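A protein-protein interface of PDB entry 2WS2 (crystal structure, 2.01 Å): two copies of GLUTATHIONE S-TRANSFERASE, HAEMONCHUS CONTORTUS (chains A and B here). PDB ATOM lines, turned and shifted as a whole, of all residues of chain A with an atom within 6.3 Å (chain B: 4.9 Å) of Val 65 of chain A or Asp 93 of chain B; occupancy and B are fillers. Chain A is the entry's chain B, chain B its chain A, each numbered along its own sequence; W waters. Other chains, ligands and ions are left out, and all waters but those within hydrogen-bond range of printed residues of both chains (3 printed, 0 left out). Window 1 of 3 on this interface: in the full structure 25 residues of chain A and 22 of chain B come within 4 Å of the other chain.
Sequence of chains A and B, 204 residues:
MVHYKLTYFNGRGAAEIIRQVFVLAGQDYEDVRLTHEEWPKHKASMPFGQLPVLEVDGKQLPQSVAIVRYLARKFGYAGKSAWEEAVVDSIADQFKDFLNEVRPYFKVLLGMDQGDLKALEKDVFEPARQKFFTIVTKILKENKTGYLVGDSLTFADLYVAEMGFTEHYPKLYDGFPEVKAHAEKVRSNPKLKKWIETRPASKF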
ATOM      1  N   ALA A  14     -12.175  -3.166 -18.884  1.00  0.00           N
ATOM      2  CA  ALA A  14     -13.169  -3.008 -19.926  1.00  0.00           C
ATOM      3  C   ALA A  14     -14.552  -3.380 -19.448  1.00  0.00           C
ATOM      4  O   ALA A  14     -15.540  -3.003 -20.063  1.00  0.00           O
ATOM      5  CB  ALA A  14     -12.771  -3.818 -21.200  1.00  0.00           C
ATOM      6  N   ILE A  18     -20.239  -2.452 -17.558  1.00  0.00           N
ATOM      7  CA  ILE A  18     -21.167  -3.603 -17.619  1.00  0.00           C
ATOM      8  C   ILE A  18     -21.530  -4.009 -16.165  1.00  0.00           C
ATOM      9  O   ILE A  18     -22.692  -4.198 -15.829  1.00  0.00           O
ATOM     10  CB  ILE A  18     -20.505  -4.841 -18.318  1.00  0.00           C
ATOM     11  CG1 ILE A  18     -20.195  -4.584 -19.800  1.00  0.00           C
ATOM     12  CG2 ILE A  18     -21.380  -6.048 -18.242  1.00  0.00           C
ATOM     13  CD1 ILE A  18     -19.286  -5.713 -20.385  1.00  0.00           C
ATOM     14  N   PRO A  52     -14.413  -8.453 -22.344  1.00  0.00           N
ATOM     15  CA  PRO A  52     -15.478  -9.241 -21.752  1.00  0.00           C
ATOM     16  C   PRO A  52     -16.359  -9.930 -22.777  1.00  0.00           C
ATOM     17  O   PRO A  52     -16.516  -9.459 -23.878  1.00  0.00           O
ATOM     18  CB  PRO A  52     -16.305  -8.191 -20.992  1.00  0.00           C
ATOM     19  CG  PRO A  52     -16.115  -6.981 -21.796  1.00  0.00           C
ATOM     20  CD  PRO A  52     -14.733  -7.016 -22.315  1.00  0.00           C
ATOM     21  N   PRO A  62     -20.093 -10.303 -27.467  1.00  0.00           N
ATOM     22  CA  PRO A  62     -18.792  -9.757 -27.213  1.00  0.00           C
ATOM     23  C   PRO A  62     -18.795  -8.209 -27.294  1.00  0.00           C
ATOM     24  O   PRO A  62     -19.810  -7.615 -27.634  1.00  0.00           O
ATOM     25  CB  PRO A  62     -17.949 -10.391 -28.323  1.00  0.00           C
ATOM     26  CG  PRO A  62     -18.894 -10.533 -29.471  1.00  0.00           C
ATOM     27  CD  PRO A  62     -20.332 -10.391 -28.928  1.00  0.00           C
ATOM     28  N   GLN A  63     -17.690  -7.593 -26.865  1.00  0.00           N
ATOM     29  CA  GLN A  63     -17.390  -6.155 -27.018  1.00  0.00           C
ATOM     30  C   GLN A  63     -18.030  -5.280 -25.915  1.00  0.00           C
ATOM     31  O   GLN A  63     -19.225  -4.981 -25.932  1.00  0.00           O
ATOM     32  CB  GLN A  63     -17.649  -5.637 -28.465  1.00  0.00           C
ATOM     33  CG  GLN A  63     -16.543  -6.078 -29.529  1.00  0.00           C
ATOM     34  CD  GLN A  63     -15.177  -5.389 -29.407  1.00  0.00           C
ATOM     35  OE1 GLN A  63     -15.018  -4.328 -28.768  1.00  0.00           O
ATOM     36  NE2 GLN A  63     -14.173  -6.005 -30.007  1.00  0.00           N
ATOM     37  N   SER A  64     -17.187  -4.891 -24.967  1.00  0.00           N
ATOM     38  CA  SER A  64     -17.612  -4.182 -23.735  1.00  0.00           C
ATOM     39  C   SER A  64     -18.681  -3.131 -23.937  1.00  0.00           C
ATOM     40  O   SER A  64     -19.639  -3.100 -23.207  1.00  0.00           O
ATOM     41  CB  SER A  64     -16.396  -3.548 -23.041  1.00  0.00           C
ATOM     42  OG  SER A  64     -15.983  -2.412 -23.768  1.00  0.00           O
ATOM     43  N   VAL A  65     -18.530  -2.276 -24.938  1.00  0.00           N
ATOM     44  CA  VAL A  65     -19.508  -1.218 -25.163  1.00  0.00           C
ATOM     45  C   VAL A  65     -20.832  -1.731 -25.814  1.00  0.00           C
ATOM     46  O   VAL A  65     -21.927  -1.281 -25.449  1.00  0.00           O
ATOM     47  CB  VAL A  65     -18.921  -0.007 -25.965  1.00  0.00           C
ATOM     48  CG1 VAL A  65     -19.980   0.991 -26.317  1.00  0.00           C
ATOM     49  CG2 VAL A  65     -17.744   0.680 -25.234  1.00  0.00           C
ATOM     50  N   ALA A  66     -20.726  -2.635 -26.792  1.00  0.00           N
ATOM     51  CA  ALA A  66     -21.912  -3.376 -27.283  1.00  0.00           C
ATOM     52  C   ALA A  66     -22.688  -3.945 -26.051  1.00  0.00           C
ATOM     53  O   ALA A  66     -23.908  -3.804 -25.915  1.00  0.00           O
ATOM     54  CB  ALA A  66     -21.463  -4.516 -28.183  1.00  0.00           C
ATOM     55  N   ILE A  67     -21.965  -4.590 -25.169  1.00  0.00           N
ATOM     56  CA  ILE A  67     -22.611  -5.256 -24.020  1.00  0.00           C
ATOM     57  C   ILE A  67     -23.254  -4.137 -23.168  1.00  0.00           C
ATOM     58  O   ILE A  67     -24.453  -4.150 -22.949  1.00  0.00           O
ATOM     59  CB  ILE A  67     -21.632  -6.077 -23.209  1.00  0.00           C
ATOM     60  CG1 ILE A  67     -21.047  -7.226 -24.020  1.00  0.00           C
ATOM     61  CG2 ILE A  67     -22.296  -6.695 -21.921  1.00  0.00           C
ATOM     62  CD1 ILE A  67     -19.786  -7.725 -23.436  1.00  0.00           C
ATOM     63  N   VAL A  68     -22.459  -3.143 -22.781  1.00  0.00           N
ATOM     64  CA  VAL A  68     -22.987  -1.999 -21.976  1.00  0.00           C
ATOM     65  C   VAL A  68     -24.286  -1.495 -22.538  1.00  0.00           C
ATOM     66  O   VAL A  68     -25.263  -1.379 -21.797  1.00  0.00           O
ATOM     67  CB  VAL A  68     -21.965  -0.841 -21.822  1.00  0.00           C
ATOM     68  CG1 VAL A  68     -22.588   0.367 -21.083  1.00  0.00           C
ATOM     69  CG2 VAL A  68     -20.779  -1.323 -21.065  1.00  0.00           C
ATOM     70  N   ARG A  69     -24.339  -1.236 -23.858  1.00  0.00           N
ATOM     71  CA  ARG A  69     -25.553  -0.686 -24.435  1.00  0.00           C
ATOM     72  C   ARG A  69     -26.731  -1.635 -24.404  1.00  0.00           C
ATOM     73  O   ARG A  69     -27.861  -1.180 -24.203  1.00  0.00           O
ATOM     74  CB  ARG A  69     -25.314  -0.107 -25.864  1.00  0.00           C
ATOM     75  CG  ARG A  69     -26.577   0.211 -26.692  1.00  0.00           C
ATOM     76  CD  ARG A  69     -26.267   0.851 -28.086  1.00  0.00           C
ATOM     77  NE  ARG A  69     -25.199   1.833 -27.950  1.00  0.00           N
ATOM     78  CZ  ARG A  69     -23.905   1.602 -28.185  1.00  0.00           C
ATOM     79  NH1 ARG A  69     -23.460   0.410 -28.623  1.00  0.00           N
ATOM     80  NH2 ARG A  69     -23.048   2.582 -27.943  1.00  0.00           N
ATOM     81  N   TYR A  70     -26.465  -2.934 -24.646  1.00  0.00           N
ATOM     82  CA  TYR A  70     -27.493  -3.992 -24.666  1.00  0.00           C
ATOM     83  C   TYR A  70     -28.180  -4.015 -23.299  1.00  0.00           C
ATOM     84  O   TYR A  70     -29.412  -3.959 -23.193  1.00  0.00           O
ATOM     85  CB  TYR A  70     -26.832  -5.347 -24.938  1.00  0.00           C
ATOM     86  CG  TYR A  70     -27.709  -6.568 -24.747  1.00  0.00           C
ATOM     87  CD1 TYR A  70     -28.569  -7.014 -25.769  1.00  0.00           C
ATOM     88  CD2 TYR A  70     -27.662  -7.302 -23.554  1.00  0.00           C
ATOM     89  CE1 TYR A  70     -29.360  -8.129 -25.601  1.00  0.00           C
ATOM     90  CE2 TYR A  70     -28.460  -8.425 -23.380  1.00  0.00           C
ATOM     91  CZ  TYR A  70     -29.308  -8.826 -24.415  1.00  0.00           C
ATOM     92  OH  TYR A  70     -30.071  -9.956 -24.252  1.00  0.00           O
ATOM     93  N   ALA A  92     -20.337   8.910 -24.637  1.00  0.00           N
ATOM     94  CA  ALA A  92     -19.435   7.829 -24.258  1.00  0.00           C
ATOM     95  C   ALA A  92     -18.373   7.519 -25.331  1.00  0.00           C
ATOM     96  O   ALA A  92     -17.250   7.074 -25.008  1.00  0.00           O
ATOM     97  CB  ALA A  92     -20.186   6.558 -23.788  1.00  0.00           C
ATOM     98  N   LYS A  96     -14.473   7.491 -24.634  1.00  0.00           N
ATOM     99  CA  LYS A  96     -13.508   6.527 -25.102  1.00  0.00           C
ATOM    100  C   LYS A  96     -12.313   7.218 -25.796  1.00  0.00           C
ATOM    101  O   LYS A  96     -11.174   6.799 -25.634  1.00  0.00           O
ATOM    102  CB  LYS A  96     -14.204   5.482 -26.014  1.00  0.00           C
ATOM    103  CG  LYS A  96     -13.376   4.969 -27.165  1.00  0.00           C
ATOM    104  CD  LYS A  96     -13.862   3.565 -27.580  1.00  0.00           C
ATOM    105  CE  LYS A  96     -13.120   2.503 -26.764  1.00  0.00           C
ATOM    106  NZ  LYS A  96     -14.012   1.477 -26.206  1.00  0.00           N
ATOM    107  N   PHE A 155     -25.538   5.268 -18.912  1.00  0.00           N
ATOM    108  CA  PHE A 155     -24.192   4.729 -18.951  1.00  0.00           C
ATOM    109  C   PHE A 155     -23.163   5.798 -19.224  1.00  0.00           C
ATOM    110  O   PHE A 155     -21.998   5.619 -18.875  1.00  0.00           O
ATOM    111  CB  PHE A 155     -24.015   3.457 -19.813  1.00  0.00           C
ATOM    112  CG  PHE A 155     -24.355   3.633 -21.268  1.00  0.00           C
ATOM    113  CD1 PHE A 155     -25.662   3.486 -21.699  1.00  0.00           C
ATOM    114  CD2 PHE A 155     -23.352   3.883 -22.215  1.00  0.00           C
ATOM    115  CE1 PHE A 155     -26.009   3.613 -23.070  1.00  0.00           C
ATOM    116  CE2 PHE A 155     -23.666   4.017 -23.577  1.00  0.00           C
ATOM    117  CZ  PHE A 155     -25.019   3.873 -24.002  1.00  0.00           C
ATOM    118  N   TYR A 159     -19.703   6.157 -17.278  1.00  0.00           N
ATOM    119  CA  TYR A 159     -18.403   6.170 -17.926  1.00  0.00           C
ATOM    120  C   TYR A 159     -17.481   7.261 -17.371  1.00  0.00           C
ATOM    121  O   TYR A 159     -16.381   6.985 -16.861  1.00  0.00           O
ATOM    122  CB  TYR A 159     -18.588   6.323 -19.454  1.00  0.00           C
ATOM    123  CG  TYR A 159     -18.655   4.955 -20.132  1.00  0.00           C
ATOM    124  CD1 TYR A 159     -17.550   4.120 -20.109  1.00  0.00           C
ATOM    125  CD2 TYR A 159     -19.824   4.497 -20.733  1.00  0.00           C
ATOM    126  CE1 TYR A 159     -17.572   2.834 -20.675  1.00  0.00           C
ATOM    127  CE2 TYR A 159     -19.865   3.195 -21.334  1.00  0.00           C
ATOM    128  CZ  TYR A 159     -18.718   2.391 -21.295  1.00  0.00           C
ATOM    129  OH  TYR A 159     -18.693   1.135 -21.848  1.00  0.00           O
ATOM    130  N   ASP B  89     -23.757  -4.011 -33.360  1.00  0.00           N
ATOM    131  CA  ASP B  89     -22.896  -3.141 -32.620  1.00  0.00           C
ATOM    132  C   ASP B  89     -21.573  -3.839 -32.367  1.00  0.00           C
ATOM    133  O   ASP B  89     -20.592  -3.267 -32.646  1.00  0.00           O
ATOM    134  CB  ASP B  89     -23.553  -2.671 -31.271  1.00  0.00           C
ATOM    135  CG  ASP B  89     -24.618  -1.592 -31.480  1.00  0.00           C
ATOM    136  OD1 ASP B  89     -24.656  -0.961 -32.574  1.00  0.00           O
ATOM    137  OD2 ASP B  89     -25.431  -1.320 -30.551  1.00  0.00           O
ATOM    138  N   SER B  90     -21.552  -5.088 -31.886  1.00  0.00           N
ATOM    139  CA  SER B  90     -20.300  -5.708 -31.423  1.00  0.00           C
ATOM    140  C   SER B  90     -19.312  -5.917 -32.574  1.00  0.00           C
ATOM    141  O   SER B  90     -18.095  -5.886 -32.378  1.00  0.00           O
ATOM    142  CB  SER B  90     -20.564  -7.076 -30.743  1.00  0.00           C
ATOM    143  OG  SER B  90     -20.784  -8.096 -31.751  1.00  0.00           O
ATOM    144  N   ILE B  91     -19.853  -6.208 -33.751  1.00  0.00           N
ATOM    145  CA  ILE B  91     -19.020  -6.346 -35.003  1.00  0.00           C
ATOM    146  C   ILE B  91     -18.440  -4.994 -35.542  1.00  0.00           C
ATOM    147  O   ILE B  91     -17.259  -4.881 -35.772  1.00  0.00           O
ATOM    148  CB  ILE B  91     -19.768  -7.111 -36.129  1.00  0.00           C
ATOM    149  CG1 ILE B  91     -20.140  -8.513 -35.624  1.00  0.00           C
ATOM    150  CG2 ILE B  91     -18.847  -7.211 -37.407  1.00  0.00           C
ATOM    151  CD1 ILE B  91     -20.978  -9.376 -36.577  1.00  0.00           C
ATOM    152  N   ALA B  92     -19.277  -3.973 -35.691  1.00  0.00           N
ATOM    153  CA  ALA B  92     -18.798  -2.567 -35.869  1.00  0.00           C
ATOM    154  C   ALA B  92     -17.730  -2.083 -34.866  1.00  0.00           C
ATOM    155  O   ALA B  92     -16.883  -1.248 -35.187  1.00  0.00           O
ATOM    156  CB  ALA B  92     -19.968  -1.592 -35.875  1.00  0.00           C
ATOM    157  N   ASP B  93     -17.802  -2.587 -33.641  1.00  0.00           N
ATOM    158  CA  ASP B  93     -16.877  -2.203 -32.595  1.00  0.00           C
ATOM    159  C   ASP B  93     -15.564  -2.952 -32.904  1.00  0.00           C
ATOM    160  O   ASP B  93     -14.469  -2.405 -32.814  1.00  0.00           O
ATOM    161  CB  ASP B  93     -17.429  -2.690 -31.277  1.00  0.00           C
ATOM    162  CG  ASP B  93     -17.878  -1.539 -30.323  1.00  0.00           C
ATOM    163  OD1 ASP B  93     -18.178  -0.373 -30.718  1.00  0.00           O
ATOM    164  OD2 ASP B  93     -17.996  -1.887 -29.158  1.00  0.00           O
ATOM    165  N   GLN B  94     -15.699  -4.233 -33.241  1.00  0.00           N
ATOM    166  CA  GLN B  94     -14.554  -5.097 -33.475  1.00  0.00           C
ATOM    167  C   GLN B  94     -13.771  -4.648 -34.725  1.00  0.00           C
ATOM    168  O   GLN B  94     -12.536  -4.673 -34.743  1.00  0.00           O
ATOM    169  CB  GLN B  94     -15.015  -6.542 -33.658  1.00  0.00           C
ATOM    170  CG  GLN B  94     -13.897  -7.505 -34.028  1.00  0.00           C
ATOM    171  CD  GLN B  94     -13.019  -7.802 -32.828  1.00  0.00           C
ATOM    172  OE1 GLN B  94     -13.445  -7.623 -31.680  1.00  0.00           O
ATOM    173  NE2 GLN B  94     -11.820  -8.276 -33.072  1.00  0.00           N
ATOM    174  N   PHE B  95     -14.501  -4.288 -35.776  1.00  0.00           N
ATOM    175  CA  PHE B  95     -13.877  -3.758 -36.996  1.00  0.00           C
ATOM    176  C   PHE B  95     -13.105  -2.482 -36.656  1.00  0.00           C
ATOM    177  O   PHE B  95     -11.938  -2.322 -37.025  1.00  0.00           O
ATOM    178  CB  PHE B  95     -14.934  -3.526 -38.092  1.00  0.00           C
ATOM    179  CG  PHE B  95     -14.462  -2.675 -39.219  1.00  0.00           C
ATOM    180  CD1 PHE B  95     -13.582  -3.186 -40.181  1.00  0.00           C
ATOM    181  CD2 PHE B  95     -14.871  -1.343 -39.321  1.00  0.00           C
ATOM    182  CE1 PHE B  95     -13.125  -2.406 -41.231  1.00  0.00           C
ATOM    183  CE2 PHE B  95     -14.430  -0.529 -40.397  1.00  0.00           C
ATOM    184  CZ  PHE B  95     -13.541  -1.070 -41.347  1.00  0.00           C
ATOM    185  N   LYS B  96     -13.741  -1.617 -35.871  1.00  0.00           N
ATOM    186  CA  LYS B  96     -13.105  -0.390 -35.423  1.00  0.00           C
ATOM    187  C   LYS B  96     -11.772  -0.646 -34.694  1.00  0.00           C
ATOM    188  O   LYS B  96     -10.818   0.092 -34.900  1.00  0.00           O
ATOM    189  CB  LYS B  96     -14.081   0.420 -34.556  1.00  0.00           C
ATOM    190  CG  LYS B  96     -13.973   1.922 -34.739  1.00  0.00           C
ATOM    191  CD  LYS B  96     -14.823   2.379 -35.934  1.00  0.00           C
ATOM    192  CE  LYS B  96     -14.641   3.835 -36.242  1.00  0.00           C
ATOM    193  NZ  LYS B  96     -15.943   4.424 -36.738  1.00  0.00           N
ATOM    194  N   ASP B  97     -11.689  -1.680 -33.851  1.00  0.00           N
ATOM    195  CA  ASP B  97     -10.419  -1.986 -33.162  1.00  0.00           C
ATOM    196  C   ASP B  97      -9.399  -2.517 -34.160  1.00  0.00           C
ATOM    197  O   ASP B  97      -8.191  -2.491 -33.911  1.00  0.00           O
ATOM    198  CB  ASP B  97     -10.599  -3.035 -32.054  1.00  0.00           C
ATOM    199  CG  ASP B  97     -11.297  -2.481 -30.805  1.00  0.00           C
ATOM    200  OD1 ASP B  97     -11.416  -1.247 -30.667  1.00  0.00           O
ATOM    201  OD2 ASP B  97     -11.723  -3.300 -29.951  1.00  0.00           O
HETATM  202  O   HOH W   1     -25.393  -3.397 -28.283  1.00  0.00           O
HETATM  203  O   HOH W   2     -20.950  -0.675 -29.367  1.00  0.00           O
HETATM  204  O   HOH W   3     -16.661  -1.807 -27.058  1.00  0.00           O
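NH1 of Arg 69 of chain A is in salt-bridge range of OD2 of Asp 89 of chain B (3.3 Å).
The side-chain amide oxygen (OE1) of Gln 94 of chain B lies within hydrogen-bond range of the side-chain amide nitrogen (NE2) of Gln 63 of chain A, 2.4 Å away.
Positions printed for both chains: 92 and 96.
Water W3 lies within hydrogen-bond range of the side-chain carboxylate of Asp 93 of chain B (2.5 Å), the backbone NH of Val 65 of chain A (2.9 Å), the side-chain hydroxyl of Ser 64 of chain A (3.4 Å) and the side-chain amide oxygen of Gln 63 of chain A (3.5 Å).
Water W1 bridges O of Ala 66 of chain A (2.8 Å) and OD2 of Asp 89 of chain B (3.1 Å).
Water W2 lies within hydrogen-bond range of the guanidinium group (NH1) of Arg 69 of chain A (2.8 Å), the side-chain carboxylate (OD1) of Asp 93 of chain B (3.1 Å) and the backbone NH (N) of Ala 66 of chain A (3.2 Å).
Val 65 of chain A touches just one residue of chain B: Asp 93.
Of the printed residues of chain B, Arg 69 of chain A touches Asp 89 (3.3 Å).
Printed residues of chain A within 4 Å of Ser 90 of chain B: Pro 62, Gln 63 and Ala 66.
Of the printed residues of chain A, Asp 93 of chain B touches Gln 63 (3.8 Å), Val 65 (3.8 Å) and Ala 66 (3.7 Å).
Printed residues of chain A within 4 Å of Gln 94 of chain B: Gln 63.
The nearest printed residue of chain B that does not touch Val 65 of chain A is Asp 89 of chain B (6.2 Å).
The nearest residue of chain A that does not touch Asp 93 of chain B is Ser 64 of chain A (5.2 Å).
The nearest printed residue of chain B that does not touch Gln 63 of chain A is Ile 91 of chain B (5.4 Å).
Among the printed residues, pairs that only touch across the chains: Pro 62 of chain A with Ser 90 of chain B, Gln 63 of chain A with Ser 90 of chain B, Gln 63 of chain A with Asp 93 of chain B, Gln 63 of chain A with Asp 97 of chain B, Val 65 of chain A with Asp 93 of chain B, Ala 66 of chain A with Ser 90 of chain B and Ala 66 of chain A with Asp 93 of chain B.
Of the 16 printed residues of chain A, 5 touch a printed residue of chain B.
Hydrophobic or aromatic side chains of chain A within 4 Å of the printed part of chain B: Pro 62, Val 65 and Ala 66.
Along chain A the printed residues that touch a printed residue of chain B span positions 62 to 69.
Among the printed residues, 9 pairs touch across the chains.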
